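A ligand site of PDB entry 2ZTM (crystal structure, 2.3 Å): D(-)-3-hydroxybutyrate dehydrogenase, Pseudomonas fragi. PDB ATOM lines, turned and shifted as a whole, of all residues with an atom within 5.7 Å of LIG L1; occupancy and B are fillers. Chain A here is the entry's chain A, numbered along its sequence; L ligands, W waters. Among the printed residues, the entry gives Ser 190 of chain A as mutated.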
ATOM      1  N   THR A  10       5.949 -19.499  20.811  1.00  0.00           N
ATOM      2  CA  THR A  10       5.578 -18.105  20.589  1.00  0.00           C
ATOM      3  C   THR A  10       4.420 -17.984  19.603  1.00  0.00           C
ATOM      4  O   THR A  10       4.298 -18.807  18.697  1.00  0.00           O
ATOM      5  CB  THR A  10       6.782 -17.284  20.056  1.00  0.00           C
ATOM      6  OG1 THR A  10       7.100 -17.697  18.728  1.00  0.00           O
ATOM      7  CG2 THR A  10       7.990 -17.490  20.937  1.00  0.00           C
ATOM      8  N   GLY A  11       3.595 -16.964  19.773  1.00  0.00           N
ATOM      9  CA  GLY A  11       2.461 -16.783  18.881  1.00  0.00           C
ATOM     10  C   GLY A  11       1.604 -18.028  18.814  1.00  0.00           C
ATOM     11  O   GLY A  11       1.133 -18.422  17.749  1.00  0.00           O
ATOM     12  N   SER A  12       1.385 -18.647  19.977  1.00  0.00           N
ATOM     13  CA  SER A  12       0.604 -19.866  20.053  1.00  0.00           C
ATOM     14  C   SER A  12      -0.840 -19.699  20.494  1.00  0.00           C
ATOM     15  O   SER A  12      -1.447 -20.631  21.020  1.00  0.00           O
ATOM     16  CB  SER A  12       1.313 -20.867  20.972  1.00  0.00           C
ATOM     17  OG  SER A  12       1.617 -20.267  22.217  1.00  0.00           O
ATOM     18  N   THR A  13      -1.409 -18.507  20.295  1.00  0.00           N
ATOM     19  CA  THR A  13      -2.800 -18.264  20.662  1.00  0.00           C
ATOM     20  C   THR A  13      -3.679 -18.330  19.419  1.00  0.00           C
ATOM     21  O   THR A  13      -4.905 -18.159  19.502  1.00  0.00           O
ATOM     22  CB  THR A  13      -2.990 -16.865  21.316  1.00  0.00           C
ATOM     23  OG1 THR A  13      -2.653 -15.837  20.364  1.00  0.00           O
ATOM     24  CG2 THR A  13      -2.129 -16.716  22.547  1.00  0.00           C
ATOM     25  N   SER A  14      -3.053 -18.582  18.279  1.00  0.00           N
ATOM     26  CA  SER A  14      -3.759 -18.646  16.996  1.00  0.00           C
ATOM     27  C   SER A  14      -3.044 -19.538  15.975  1.00  0.00           C
ATOM     28  O   SER A  14      -1.872 -19.889  16.155  1.00  0.00           O
ATOM     29  CB  SER A  14      -3.878 -17.224  16.426  1.00  0.00           C
ATOM     30  OG  SER A  14      -4.425 -17.221  15.119  1.00  0.00           O
ATOM     31  N   GLY A  15      -3.785 -19.903  14.934  1.00  0.00           N
ATOM     32  CA  GLY A  15      -3.268 -20.727  13.857  1.00  0.00           C
ATOM     33  C   GLY A  15      -2.208 -21.782  14.117  1.00  0.00           C
ATOM     34  O   GLY A  15      -2.375 -22.672  14.945  1.00  0.00           O
ATOM     35  N   ILE A  16      -1.116 -21.691  13.374  1.00  0.00           N
ATOM     36  CA  ILE A  16      -0.013 -22.636  13.472  1.00  0.00           C
ATOM     37  C   ILE A  16       0.541 -22.830  14.881  1.00  0.00           C
ATOM     38  O   ILE A  16       0.828 -23.950  15.290  1.00  0.00           O
ATOM     39  CB  ILE A  16       1.143 -22.244  12.532  1.00  0.00           C
ATOM     40  CG1 ILE A  16       0.646 -22.232  11.085  1.00  0.00           C
ATOM     41  CG2 ILE A  16       2.321 -23.193  12.702  1.00  0.00           C
ATOM     42  CD1 ILE A  16       1.744 -21.897  10.064  1.00  0.00           C
ATOM     43  N   GLY A  17       0.724 -21.732  15.602  1.00  0.00           N
ATOM     44  CA  GLY A  17       1.245 -21.821  16.953  1.00  0.00           C
ATOM     45  C   GLY A  17       0.324 -22.626  17.853  1.00  0.00           C
ATOM     46  O   GLY A  17       0.778 -23.471  18.628  1.00  0.00           O
ATOM     47  N   ASN A  34       1.664 -18.001  24.240  1.00  0.00           N
ATOM     48  CA  ASN A  34       2.096 -16.631  23.994  1.00  0.00           C
ATOM     49  C   ASN A  34       1.383 -16.117  22.763  1.00  0.00           C
ATOM     50  O   ASN A  34       1.072 -16.873  21.855  1.00  0.00           O
ATOM     51  CB  ASN A  34       3.615 -16.605  23.805  1.00  0.00           C
ATOM     52  CG  ASN A  34       4.108 -15.316  23.148  1.00  0.00           C
ATOM     53  OD1 ASN A  34       4.082 -15.178  21.924  1.00  0.00           O
ATOM     54  ND2 ASN A  34       4.557 -14.369  23.972  1.00  0.00           N
ATOM     55  N   GLY A  35       1.094 -14.821  22.738  1.00  0.00           N
ATOM     56  CA  GLY A  35       0.419 -14.275  21.594  1.00  0.00           C
ATOM     57  C   GLY A  35      -0.696 -13.340  22.000  1.00  0.00           C
ATOM     58  O   GLY A  35      -0.920 -13.108  23.182  1.00  0.00           O
ATOM     59  N   PHE A  36      -1.393 -12.820  21.002  1.00  0.00           N
ATOM     60  CA  PHE A  36      -2.484 -11.894  21.274  1.00  0.00           C
ATOM     61  C   PHE A  36      -3.845 -12.411  20.842  1.00  0.00           C
ATOM     62  O   PHE A  36      -4.003 -13.577  20.527  1.00  0.00           O
ATOM     63  CB  PHE A  36      -2.170 -10.542  20.625  1.00  0.00           C
ATOM     64  CG  PHE A  36      -0.923  -9.899  21.163  1.00  0.00           C
ATOM     65  CD1 PHE A  36      -0.726  -9.803  22.537  1.00  0.00           C
ATOM     66  CD2 PHE A  36       0.043  -9.397  20.298  1.00  0.00           C
ATOM     67  CE1 PHE A  36       0.426  -9.213  23.043  1.00  0.00           C
ATOM     68  CE2 PHE A  36       1.194  -8.808  20.804  1.00  0.00           C
ATOM     69  CZ  PHE A  36       1.392  -8.712  22.178  1.00  0.00           C
ATOM     70  N   GLY A  37      -4.827 -11.510  20.847  1.00  0.00           N
ATOM     71  CA  GLY A  37      -6.180 -11.893  20.511  1.00  0.00           C
ATOM     72  C   GLY A  37      -7.075 -11.527  21.690  1.00  0.00           C
ATOM     73  O   GLY A  37      -6.788 -10.587  22.425  1.00  0.00           O
ATOM     74  N   ALA A  62       4.012 -11.558  26.391  1.00  0.00           N
ATOM     75  CA  ALA A  62       5.116 -10.696  25.988  1.00  0.00           C
ATOM     76  C   ALA A  62       5.005 -10.287  24.516  1.00  0.00           C
ATOM     77  O   ALA A  62       4.641 -11.096  23.662  1.00  0.00           O
ATOM     78  CB  ALA A  62       6.433 -11.401  26.249  1.00  0.00           C
ATOM     79  N   ASP A  63       5.307  -9.019  24.225  1.00  0.00           N
ATOM     80  CA  ASP A  63       5.272  -8.478  22.866  1.00  0.00           C
ATOM     81  C   ASP A  63       6.658  -8.756  22.273  1.00  0.00           C
ATOM     82  O   ASP A  63       7.605  -8.023  22.537  1.00  0.00           O
ATOM     83  CB  ASP A  63       5.032  -6.974  22.904  1.00  0.00           C
ATOM     84  CG  ASP A  63       5.023  -6.345  21.525  1.00  0.00           C
ATOM     85  OD1 ASP A  63       5.629  -6.917  20.592  1.00  0.00           O
ATOM     86  OD2 ASP A  63       4.414  -5.259  21.370  1.00  0.00           O
ATOM     87  N   LEU A  64       6.769  -9.812  21.468  1.00  0.00           N
ATOM     88  CA  LEU A  64       8.038 -10.238  20.887  1.00  0.00           C
ATOM     89  C   LEU A  64       8.707  -9.295  19.893  1.00  0.00           C
ATOM     90  O   LEU A  64       9.749  -9.643  19.323  1.00  0.00           O
ATOM     91  CB  LEU A  64       7.861 -11.615  20.245  1.00  0.00           C
ATOM     92  CG  LEU A  64       7.265 -12.631  21.222  1.00  0.00           C
ATOM     93  CD1 LEU A  64       7.253 -14.005  20.589  1.00  0.00           C
ATOM     94  CD2 LEU A  64       8.069 -12.632  22.534  1.00  0.00           C
ATOM     95  N   SER A  65       8.133  -8.118  19.690  1.00  0.00           N
ATOM     96  CA  SER A  65       8.733  -7.154  18.775  1.00  0.00           C
ATOM     97  C   SER A  65       9.863  -6.438  19.508  1.00  0.00           C
ATOM     98  O   SER A  65      10.440  -5.502  18.982  1.00  0.00           O
ATOM     99  CB  SER A  65       7.697  -6.137  18.312  1.00  0.00           C
ATOM    100  OG  SER A  65       7.383  -5.242  19.356  1.00  0.00           O
ATOM    101  N   ASN A  90       7.596 -19.289  16.601  1.00  0.00           N
ATOM    102  CA  ASN A  90       6.550 -19.252  15.587  1.00  0.00           C
ATOM    103  C   ASN A  90       5.927 -17.889  15.278  1.00  0.00           C
ATOM    104  O   ASN A  90       5.534 -17.624  14.141  1.00  0.00           O
ATOM    105  CB  ASN A  90       5.453 -20.228  16.017  1.00  0.00           C
ATOM    106  CG  ASN A  90       4.169 -20.052  15.237  1.00  0.00           C
ATOM    107  OD1 ASN A  90       4.016 -20.576  14.130  1.00  0.00           O
ATOM    108  ND2 ASN A  90       3.233 -19.286  15.802  1.00  0.00           N
ATOM    109  N   ALA A  91       5.808 -17.024  16.283  1.00  0.00           N
ATOM    110  CA  ALA A  91       5.190 -15.708  16.082  1.00  0.00           C
ATOM    111  C   ALA A  91       5.707 -14.997  14.825  1.00  0.00           C
ATOM    112  O   ALA A  91       6.912 -14.919  14.591  1.00  0.00           O
ATOM    113  CB  ALA A  91       5.422 -14.844  17.317  1.00  0.00           C
ATOM    114  N   GLY A  92       4.768 -14.474  14.033  1.00  0.00           N
ATOM    115  CA  GLY A  92       5.114 -13.777  12.809  1.00  0.00           C
ATOM    116  C   GLY A  92       3.980 -12.932  12.222  1.00  0.00           C
ATOM    117  O   GLY A  92       2.810 -13.161  12.533  1.00  0.00           O
ATOM    118  N   ILE A  93       4.328 -11.959  11.378  1.00  0.00           N
ATOM    119  CA  ILE A  93       3.346 -11.090  10.739  1.00  0.00           C
ATOM    120  C   ILE A  93       3.666 -10.914   9.261  1.00  0.00           C
ATOM    121  O   ILE A  93       4.737 -11.305   8.798  1.00  0.00           O
ATOM    122  CB  ILE A  93       3.320  -9.682  11.365  1.00  0.00           C
ATOM    123  CG1 ILE A  93       4.740  -9.124  11.412  1.00  0.00           C
ATOM    124  CG2 ILE A  93       2.679  -9.743  12.744  1.00  0.00           C
ATOM    125  CD1 ILE A  93       4.836  -7.736  11.981  1.00  0.00           C
ATOM    126  N   LEU A 113      10.155  -8.977  14.452  1.00  0.00           N
ATOM    127  CA  LEU A 113       9.375 -10.125  14.903  1.00  0.00           C
ATOM    128  C   LEU A 113       9.692 -11.446  14.189  1.00  0.00           C
ATOM    129  O   LEU A 113       9.954 -12.466  14.836  1.00  0.00           O
ATOM    130  CB  LEU A 113       7.876  -9.844  14.751  1.00  0.00           C
ATOM    131  CG  LEU A 113       6.974 -10.972  15.258  1.00  0.00           C
ATOM    132  CD1 LEU A 113       7.213 -11.199  16.746  1.00  0.00           C
ATOM    133  CD2 LEU A 113       5.516 -10.600  15.008  1.00  0.00           C
ATOM    134  N   ASN A 114       9.678 -11.416  12.862  1.00  0.00           N
ATOM    135  CA  ASN A 114       9.933 -12.617  12.061  1.00  0.00           C
ATOM    136  C   ASN A 114      11.355 -13.141  12.095  1.00  0.00           C
ATOM    137  O   ASN A 114      11.586 -14.330  11.863  1.00  0.00           O
ATOM    138  CB  ASN A 114       9.492 -12.388  10.613  1.00  0.00           C
ATOM    139  CG  ASN A 114       7.999 -12.196  10.491  1.00  0.00           C
ATOM    140  OD1 ASN A 114       7.350 -11.644  11.380  1.00  0.00           O
ATOM    141  ND2 ASN A 114       7.438 -12.654   9.373  1.00  0.00           N
ATOM    142  N   ILE A 140       9.654 -21.715  12.942  1.00  0.00           N
ATOM    143  CA  ILE A 140       8.652 -21.795  11.907  1.00  0.00           C
ATOM    144  C   ILE A 140       8.991 -20.764  10.838  1.00  0.00           C
ATOM    145  O   ILE A 140       8.691 -19.569  10.970  1.00  0.00           O
ATOM    146  CB  ILE A 140       7.244 -21.512  12.451  1.00  0.00           C
ATOM    147  CG1 ILE A 140       6.952 -22.416  13.648  1.00  0.00           C
ATOM    148  CG2 ILE A 140       6.219 -21.734  11.351  1.00  0.00           C
ATOM    149  CD1 ILE A 140       7.044 -23.897  13.343  1.00  0.00           C
ATOM    150  N   ALA A 141       9.663 -21.219   9.787  1.00  0.00           N
ATOM    151  CA  ALA A 141      10.029 -20.353   8.688  1.00  0.00           C
ATOM    152  C   ALA A 141       8.874 -20.327   7.701  1.00  0.00           C
ATOM    153  O   ALA A 141       7.772 -19.907   8.041  1.00  0.00           O
ATOM    154  CB  ALA A 141      11.305 -20.856   8.006  1.00  0.00           C
ATOM    155  N   SER A 142       9.130 -20.806   6.482  1.00  0.00           N
ATOM    156  CA  SER A 142       8.126 -20.795   5.425  1.00  0.00           C
ATOM    157  C   SER A 142       8.769 -21.219   4.112  1.00  0.00           C
ATOM    158  O   SER A 142       9.996 -21.247   3.999  1.00  0.00           O
ATOM    159  CB  SER A 142       7.590 -19.370   5.286  1.00  0.00           C
ATOM    160  OG  SER A 142       6.879 -19.190   4.075  1.00  0.00           O
ATOM    161  N   ALA A 143       7.941 -21.553   3.130  1.00  0.00           N
ATOM    162  CA  ALA A 143       8.483 -21.912   1.825  1.00  0.00           C
ATOM    163  C   ALA A 143       9.222 -20.645   1.382  1.00  0.00           C
ATOM    164  O   ALA A 143      10.187 -20.689   0.605  1.00  0.00           O
ATOM    165  CB  ALA A 143       7.343 -22.235   0.846  1.00  0.00           C
ATOM    166  N   TYR A 155       9.130 -10.041   4.399  1.00  0.00           N
ATOM    167  CA  TYR A 155       8.793 -11.393   4.805  1.00  0.00           C
ATOM    168  C   TYR A 155       9.785 -12.398   4.248  1.00  0.00           C
ATOM    169  O   TYR A 155      10.356 -13.205   4.993  1.00  0.00           O
ATOM    170  CB  TYR A 155       7.369 -11.727   4.344  1.00  0.00           C
ATOM    171  CG  TYR A 155       6.809 -13.022   4.892  1.00  0.00           C
ATOM    172  CD1 TYR A 155       7.095 -14.245   4.282  1.00  0.00           C
ATOM    173  CD2 TYR A 155       5.970 -13.033   6.015  1.00  0.00           C
ATOM    174  CE1 TYR A 155       6.547 -15.443   4.755  1.00  0.00           C
ATOM    175  CE2 TYR A 155       5.424 -14.215   6.505  1.00  0.00           C
ATOM    176  CZ  TYR A 155       5.723 -15.420   5.870  1.00  0.00           C
ATOM    177  OH  TYR A 155       5.198 -16.602   6.351  1.00  0.00           O
ATOM    178  N   LYS A 159      12.297 -14.560   6.551  1.00  0.00           N
ATOM    179  CA  LYS A 159      12.181 -16.009   6.530  1.00  0.00           C
ATOM    180  C   LYS A 159      13.473 -16.663   6.059  1.00  0.00           C
ATOM    181  O   LYS A 159      13.855 -17.726   6.544  1.00  0.00           O
ATOM    182  CB  LYS A 159      10.992 -16.450   5.674  1.00  0.00           C
ATOM    183  CG  LYS A 159       9.648 -16.093   6.301  1.00  0.00           C
ATOM    184  CD  LYS A 159       9.506 -16.711   7.707  1.00  0.00           C
ATOM    185  CE  LYS A 159       8.131 -16.498   8.297  1.00  0.00           C
ATOM    186  NZ  LYS A 159       7.969 -17.197   9.616  1.00  0.00           N
ATOM    187  N   CYS A 184       9.077 -25.390   7.106  1.00  0.00           N
ATOM    188  CA  CYS A 184       8.803 -24.399   6.084  1.00  0.00           C
ATOM    189  C   CYS A 184       7.478 -24.722   5.416  1.00  0.00           C
ATOM    190  O   CYS A 184       7.443 -25.332   4.347  1.00  0.00           O
ATOM    191  CB  CYS A 184       9.942 -24.387   5.052  1.00  0.00           C
ATOM    192  SG  CYS A 184      11.547 -23.879   5.727  1.00  0.00           S
ATOM    193  N   PRO A 185       6.368 -24.306   6.047  1.00  0.00           N
ATOM    194  CA  PRO A 185       5.015 -24.546   5.555  1.00  0.00           C
ATOM    195  C   PRO A 185       4.648 -23.795   4.294  1.00  0.00           C
ATOM    196  O   PRO A 185       5.233 -22.764   3.971  1.00  0.00           O
ATOM    197  CB  PRO A 185       4.129 -24.090   6.731  1.00  0.00           C
ATOM    198  CG  PRO A 185       5.031 -24.146   7.917  1.00  0.00           C
ATOM    199  CD  PRO A 185       6.329 -23.627   7.352  1.00  0.00           C
ATOM    200  N   GLY A 186       3.677 -24.344   3.570  1.00  0.00           N
ATOM    201  CA  GLY A 186       3.168 -23.705   2.377  1.00  0.00           C
ATOM    202  C   GLY A 186       1.893 -23.073   2.872  1.00  0.00           C
ATOM    203  O   GLY A 186       1.729 -22.930   4.085  1.00  0.00           O
ATOM    204  N   TRP A 187       0.971 -22.715   1.996  1.00  0.00           N
ATOM    205  CA  TRP A 187      -0.272 -22.101   2.461  1.00  0.00           C
ATOM    206  C   TRP A 187      -0.955 -22.873   3.593  1.00  0.00           C
ATOM    207  O   TRP A 187      -1.108 -24.097   3.539  1.00  0.00           O
ATOM    208  CB  TRP A 187      -1.270 -21.961   1.308  1.00  0.00           C
ATOM    209  CG  TRP A 187      -0.865 -21.059   0.201  1.00  0.00           C
ATOM    210  CD1 TRP A 187      -0.726 -21.384  -1.117  1.00  0.00           C
ATOM    211  CD2 TRP A 187      -0.601 -19.650   0.288  1.00  0.00           C
ATOM    212  NE1 TRP A 187      -0.407 -20.278  -1.861  1.00  0.00           N
ATOM    213  CE2 TRP A 187      -0.316 -19.194  -1.027  1.00  0.00           C
ATOM    214  CE3 TRP A 187      -0.580 -18.726   1.338  1.00  0.00           C
ATOM    215  CZ2 TRP A 187      -0.020 -17.857  -1.306  1.00  0.00           C
ATOM    216  CZ3 TRP A 187      -0.284 -17.389   1.059  1.00  0.00           C
ATOM    217  CH2 TRP A 187      -0.005 -16.973  -0.261  1.00  0.00           C
ATOM    218  N   VAL A 188      -1.363 -22.136   4.632  1.00  0.00           N
ATOM    219  CA  VAL A 188      -2.084 -22.668   5.782  1.00  0.00           C
ATOM    220  C   VAL A 188      -3.195 -21.647   5.925  1.00  0.00           C
ATOM    221  O   VAL A 188      -2.930 -20.465   6.153  1.00  0.00           O
ATOM    222  CB  VAL A 188      -1.243 -22.671   7.067  1.00  0.00           C
ATOM    223  CG1 VAL A 188      -2.090 -23.114   8.250  1.00  0.00           C
ATOM    224  CG2 VAL A 188      -0.057 -23.596   6.903  1.00  0.00           C
ATOM    225  N   ARG A 189      -4.449 -22.068   5.768  1.00  0.00           N
ATOM    226  CA  ARG A 189      -5.560 -21.128   5.814  1.00  0.00           C
ATOM    227  C   ARG A 189      -5.841 -20.461   7.169  1.00  0.00           C
ATOM    228  O   ARG A 189      -6.971 -20.491   7.664  1.00  0.00           O
ATOM    229  CB  ARG A 189      -6.817 -21.791   5.265  1.00  0.00           C
ATOM    230  CG  ARG A 189      -7.929 -20.798   4.970  1.00  0.00           C
ATOM    231  CD  ARG A 189      -8.935 -21.334   3.979  1.00  0.00           C
ATOM    232  NE  ARG A 189      -9.878 -20.297   3.595  1.00  0.00           N
ATOM    233  CZ  ARG A 189     -10.657 -20.354   2.513  1.00  0.00           C
ATOM    234  NH1 ARG A 189     -11.491 -19.367   2.250  1.00  0.00           N
ATOM    235  NH2 ARG A 189     -10.592 -21.405   1.703  1.00  0.00           N
ATOM    236  N   SER A 190      -4.812 -19.826   7.734  1.00  0.00           N
ATOM    237  CA  SER A 190      -4.936 -19.110   9.004  1.00  0.00           C
ATOM    238  C   SER A 190      -5.419 -17.690   8.695  1.00  0.00           C
ATOM    239  O   SER A 190      -5.674 -17.360   7.543  1.00  0.00           O
ATOM    240  CB  SER A 190      -3.581 -19.042   9.709  1.00  0.00           C
ATOM    241  OG  SER A 190      -2.716 -18.161   8.999  1.00  0.00           O
ATOM    242  N   PRO A 191      -5.577 -16.837   9.733  1.00  0.00           N
ATOM    243  CA  PRO A 191      -6.031 -15.469   9.441  1.00  0.00           C
ATOM    244  C   PRO A 191      -5.009 -14.699   8.602  1.00  0.00           C
ATOM    245  O   PRO A 191      -5.375 -13.780   7.866  1.00  0.00           O
ATOM    246  CB  PRO A 191      -6.205 -14.871  10.834  1.00  0.00           C
ATOM    247  CG  PRO A 191      -6.575 -16.063  11.666  1.00  0.00           C
ATOM    248  CD  PRO A 191      -5.610 -17.103  11.179  1.00  0.00           C
ATOM    249  N   LEU A 192      -3.741 -15.089   8.710  1.00  0.00           N
ATOM    250  CA  LEU A 192      -2.661 -14.443   7.949  1.00  0.00           C
ATOM    251  C   LEU A 192      -2.842 -14.648   6.436  1.00  0.00           C
ATOM    252  O   LEU A 192      -2.426 -13.808   5.635  1.00  0.00           O
ATOM    253  CB  LEU A 192      -1.293 -14.977   8.401  1.00  0.00           C
ATOM    254  CG  LEU A 192      -0.041 -14.284   7.825  1.00  0.00           C
ATOM    255  CD1 LEU A 192       1.117 -14.432   8.787  1.00  0.00           C
ATOM    256  CD2 LEU A 192       0.293 -14.870   6.463  1.00  0.00           C
ATOM    257  N   VAL A 193      -3.465 -15.755   6.057  1.00  0.00           N
ATOM    258  CA  VAL A 193      -3.701 -16.048   4.646  1.00  0.00           C
ATOM    259  C   VAL A 193      -5.106 -15.660   4.184  1.00  0.00           C
ATOM    260  O   VAL A 193      -5.315 -15.361   3.012  1.00  0.00           O
ATOM    261  CB  VAL A 193      -3.477 -17.550   4.338  1.00  0.00           C
ATOM    262  CG1 VAL A 193      -4.070 -17.907   2.977  1.00  0.00           C
ATOM    263  CG2 VAL A 193      -2.005 -17.851   4.348  1.00  0.00           C
HETATM  264  P1  LIG L   1      -1.734 -16.130  12.790  1.00  0.00           P
HETATM  265  O1  LIG L   1      -1.930 -14.660  12.660  1.00  0.00           O
HETATM  266  O2  LIG L   1      -2.938 -17.022  12.786  1.00  0.00           O
HETATM  267  O3  LIG L   1      -0.851 -16.368  14.087  1.00  0.00           O
HETATM  268  C1  LIG L   1       0.231 -15.465  14.448  1.00  0.00           C
HETATM  269  C2  LIG L   1       0.407 -15.480  15.954  1.00  0.00           C
HETATM  270  O4  LIG L   1       1.485 -14.506  16.188  1.00  0.00           O
HETATM  271  C3  LIG L   1      -0.832 -14.942  16.745  1.00  0.00           C
HETATM  272  O5  LIG L   1      -1.158 -15.906  17.794  1.00  0.00           O
HETATM  273  C4  LIG L   1      -0.399 -13.619  17.320  1.00  0.00           C
HETATM  274  O6  LIG L   1      -1.006 -13.150  18.463  1.00  0.00           O
HETATM  275  C5  LIG L   1       1.136 -13.814  17.379  1.00  0.00           C
HETATM  276  N1  LIG L   1       1.774 -12.506  17.332  1.00  0.00           N
HETATM  277  C6  LIG L   1       1.740 -11.455  16.427  1.00  0.00           C
HETATM  278  N2  LIG L   1       2.480 -10.429  16.786  1.00  0.00           N
HETATM  279  C7  LIG L   1       3.055 -10.739  17.954  1.00  0.00           C
HETATM  280  C8  LIG L   1       3.967 -10.021  18.848  1.00  0.00           C
HETATM  281  N3  LIG L   1       4.409  -8.814  18.590  1.00  0.00           N
HETATM  282  N4  LIG L   1       4.342 -10.729  19.997  1.00  0.00           N
HETATM  283  C9  LIG L   1       3.928 -11.971  20.326  1.00  0.00           C
HETATM  284  N5  LIG L   1       3.054 -12.693  19.509  1.00  0.00           N
HETATM  285  C10 LIG L   1       2.638 -12.039  18.329  1.00  0.00           C
HETATM  286  O7  LIG L   1      -0.797 -16.648  11.615  1.00  0.00           O
HETATM  287  P2  LIG L   1      -0.066 -18.092  11.299  1.00  0.00           P
HETATM  288  O8  LIG L   1      -0.229 -18.351   9.867  1.00  0.00           O
HETATM  289  O9  LIG L   1      -0.514 -19.092  12.311  1.00  0.00           O
HETATM  290  O10 LIG L   1       1.466 -17.648  11.535  1.00  0.00           O
HETATM  291  C11 LIG L   1       2.369 -18.484  12.310  1.00  0.00           C
HETATM  292  C12 LIG L   1       3.714 -18.541  11.674  1.00  0.00           C
HETATM  293  O11 LIG L   1       3.608 -19.337  10.406  1.00  0.00           O
HETATM  294  C13 LIG L   1       4.288 -17.144  11.219  1.00  0.00           C
HETATM  295  O12 LIG L   1       5.690 -17.041  11.557  1.00  0.00           O
HETATM  296  C14 LIG L   1       4.086 -17.148   9.698  1.00  0.00           C
HETATM  297  O13 LIG L   1       4.910 -16.242   9.031  1.00  0.00           O
HETATM  298  C15 LIG L   1       4.349 -18.662   9.378  1.00  0.00           C
HETATM  299  N6  LIG L   1       3.874 -19.109   8.011  1.00  0.00           N
HETATM  300  C16 LIG L   1       2.481 -18.895   7.654  1.00  0.00           C
HETATM  301  C17 LIG L   1       1.841 -19.706   6.805  1.00  0.00           C
HETATM  302  C18 LIG L   1       0.393 -19.484   6.411  1.00  0.00           C
HETATM  303  O14 LIG L   1       0.088 -19.612   5.210  1.00  0.00           O
HETATM  304  N7  LIG L   1      -0.518 -19.175   7.331  1.00  0.00           N
HETATM  305  C19 LIG L   1       2.552 -20.902   6.175  1.00  0.00           C
HETATM  306  C20 LIG L   1       4.058 -20.725   6.165  1.00  0.00           C
HETATM  307  C21 LIG L   1       4.656 -20.040   7.264  1.00  0.00           C
HETATM  308  C1  LG2 L   2       2.656 -17.098   3.842  1.00  0.00           C
HETATM  309  C2  LG2 L   2       3.623 -18.135   3.238  1.00  0.00           C
HETATM  310  O1  LG2 L   2       4.611 -18.379   4.240  1.00  0.00           O
HETATM  311  C3  LG2 L   2       2.820 -19.366   2.798  1.00  0.00           C
HETATM  312  C4  LG2 L   2       2.659 -15.756   3.100  1.00  0.00           C
HETATM  313  O2  LG2 L   2       3.446 -15.585   2.147  1.00  0.00           O
HETATM  314  O3  LG2 L   2       1.875 -14.871   3.475  1.00  0.00           O
HETATM  315  O   HOH W   1       0.039 -12.376  11.945  1.00  0.00           O
HETATM  316  O   HOH W   2       2.243  -7.929  15.843  1.00  0.00           O
HETATM  317  O   HOH W   3       0.543 -18.679  15.050  1.00  0.00           O
HETATM  318  O   HOH W   4      -3.741 -12.365  17.067  1.00  0.00           O
HETATM  319  O   HOH W   5      -3.535 -13.156  14.479  1.00  0.00           O
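The backbone NH (N) of Phe 36 lies within hydrogen-bond range of an oxygen (O6) of LIG L1 (2.6 Å). OG of Ser 190 is in hydrogen-bond range of O8 of LIG L1 (2.6 Å). O12 of LIG L1 sits at hydrogen-bond distance from O of Asn 90 (2.7 Å). An oxygen (O13) of LIG L1 sits at hydrogen-bond distance from the side-chain hydroxyl of Tyr 155, at 2.7 Å. The backbone NH of Ser 14 lies within hydrogen-bond range of an oxygen (O5) of LIG L1 (3.3 Å). An oxygen (O2) of LIG L1 lies within hydrogen-bond range of the side-chain hydroxyl (OG) of Ser 14 (2.8 Å). An oxygen (O9) of LIG L1 sits at hydrogen-bond distance from the backbone NH (N) of Ile 16 (2.9 Å). An oxygen (O14) of LIG L1 is in hydrogen-bond range of the backbone NH of Val 188 (3.0 Å). O of Val 188 is in hydrogen-bond range of N7 of LIG L1, 3.0 Å away. An oxygen (O5) of LIG L1 is in hydrogen-bond range of the side-chain hydroxyl (OG1) of Thr 13 (3.0 Å). The backbone NH (N) of Leu 64 is in hydrogen-bond range of a nitrogen (N4) of LIG L1, at 3.0 Å. An oxygen (O12) of LIG L1 lies within hydrogen-bond range of the side-chain amino group (NZ) of Lys 159. N3 of LIG L1 is in hydrogen-bond range of OD1 of Asp 63. An oxygen (O5) of LIG L1 sits at hydrogen-bond distance from the backbone carbonyl oxygen (O) of Gly 11, 3.4 Å away. The side-chain hydroxyl of Tyr 155 lies within hydrogen-bond range of an oxygen (O1) of LG2 L2 (2.8 Å). O1 of LG2 L2 is in hydrogen-bond range of OG of Ser 142 (2.4 Å).
The side-chain hydroxyl of Ser 190 sits close to the backbone NH of Leu 192, at 3.3 Å. The side-chain hydroxyl (OG1) of Thr 10 is in hydrogen-bond range of the backbone NH (N) of Asn 90 (2.7 Å). N of Thr 13 lies close to O of Asn 34. The side-chain carboxylate (OD1) of Asp 63 is in hydrogen-bond range of the side-chain hydroxyl (OG) of Ser 65. O of Pro 185 lies within hydrogen-bond range of N of Ala 143 (3.1 Å). The side-chain amide oxygen (OD1) of Asn 34 lies within hydrogen-bond range of the backbone NH (N) of Gly 11 (2.8 Å). N of Ser 12 sits at hydrogen-bond distance from O of Asn 34. The backbone NH (N) of Ala 91 lies within hydrogen-bond range of the side-chain hydroxyl (OG1) of Thr 10, 2.8 Å away.
Water W1 lies within hydrogen-bond range of the backbone carbonyl oxygen (O) of Gly 92 (2.9 Å) and an oxygen (O1) of LIG L1 (3.1 Å).
CA of Gly 15 touches O9 of LIG L1, at 3.6 Å. Asn 34 touches LIG L1. Gly 35 touches LIG L1 (C to O6, 3.6 Å). Ala 62 touches LIG L1 (O to C9, 3.5 Å). Ser 65 touches LIG L1 (N to N3, 3.9 Å). Ala 91 touches LIG L1. Gly 92 touches LIG L1. Leu 113 touches LIG L1 (CD2 to N2, 3.5 Å). CG2 of Ile 140 touches O11 of LIG L1, 3.7 Å away. O of Ala 141 touches C21 of LIG L1 (3.2 Å). CB of Ser 142 touches C21 of LIG L1, at 3.6 Å. O of Pro 185 touches C20 of LIG L1 (3.2 Å). Gly 186 touches LIG L1 (O to C19, 3.0 Å). Trp 187 touches LIG L1. CD of Pro 191 touches O2 of LIG L1 (3.1 Å). CB of Leu 192 touches O7 of LIG L1, 3.7 Å away. Val 193 touches LIG L1. Of the 38 residues printed, 29 come within 4 Å of LIG L1. The nearest printed residue that does not touch LIG L1 is Ile 93 (4.1 Å).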
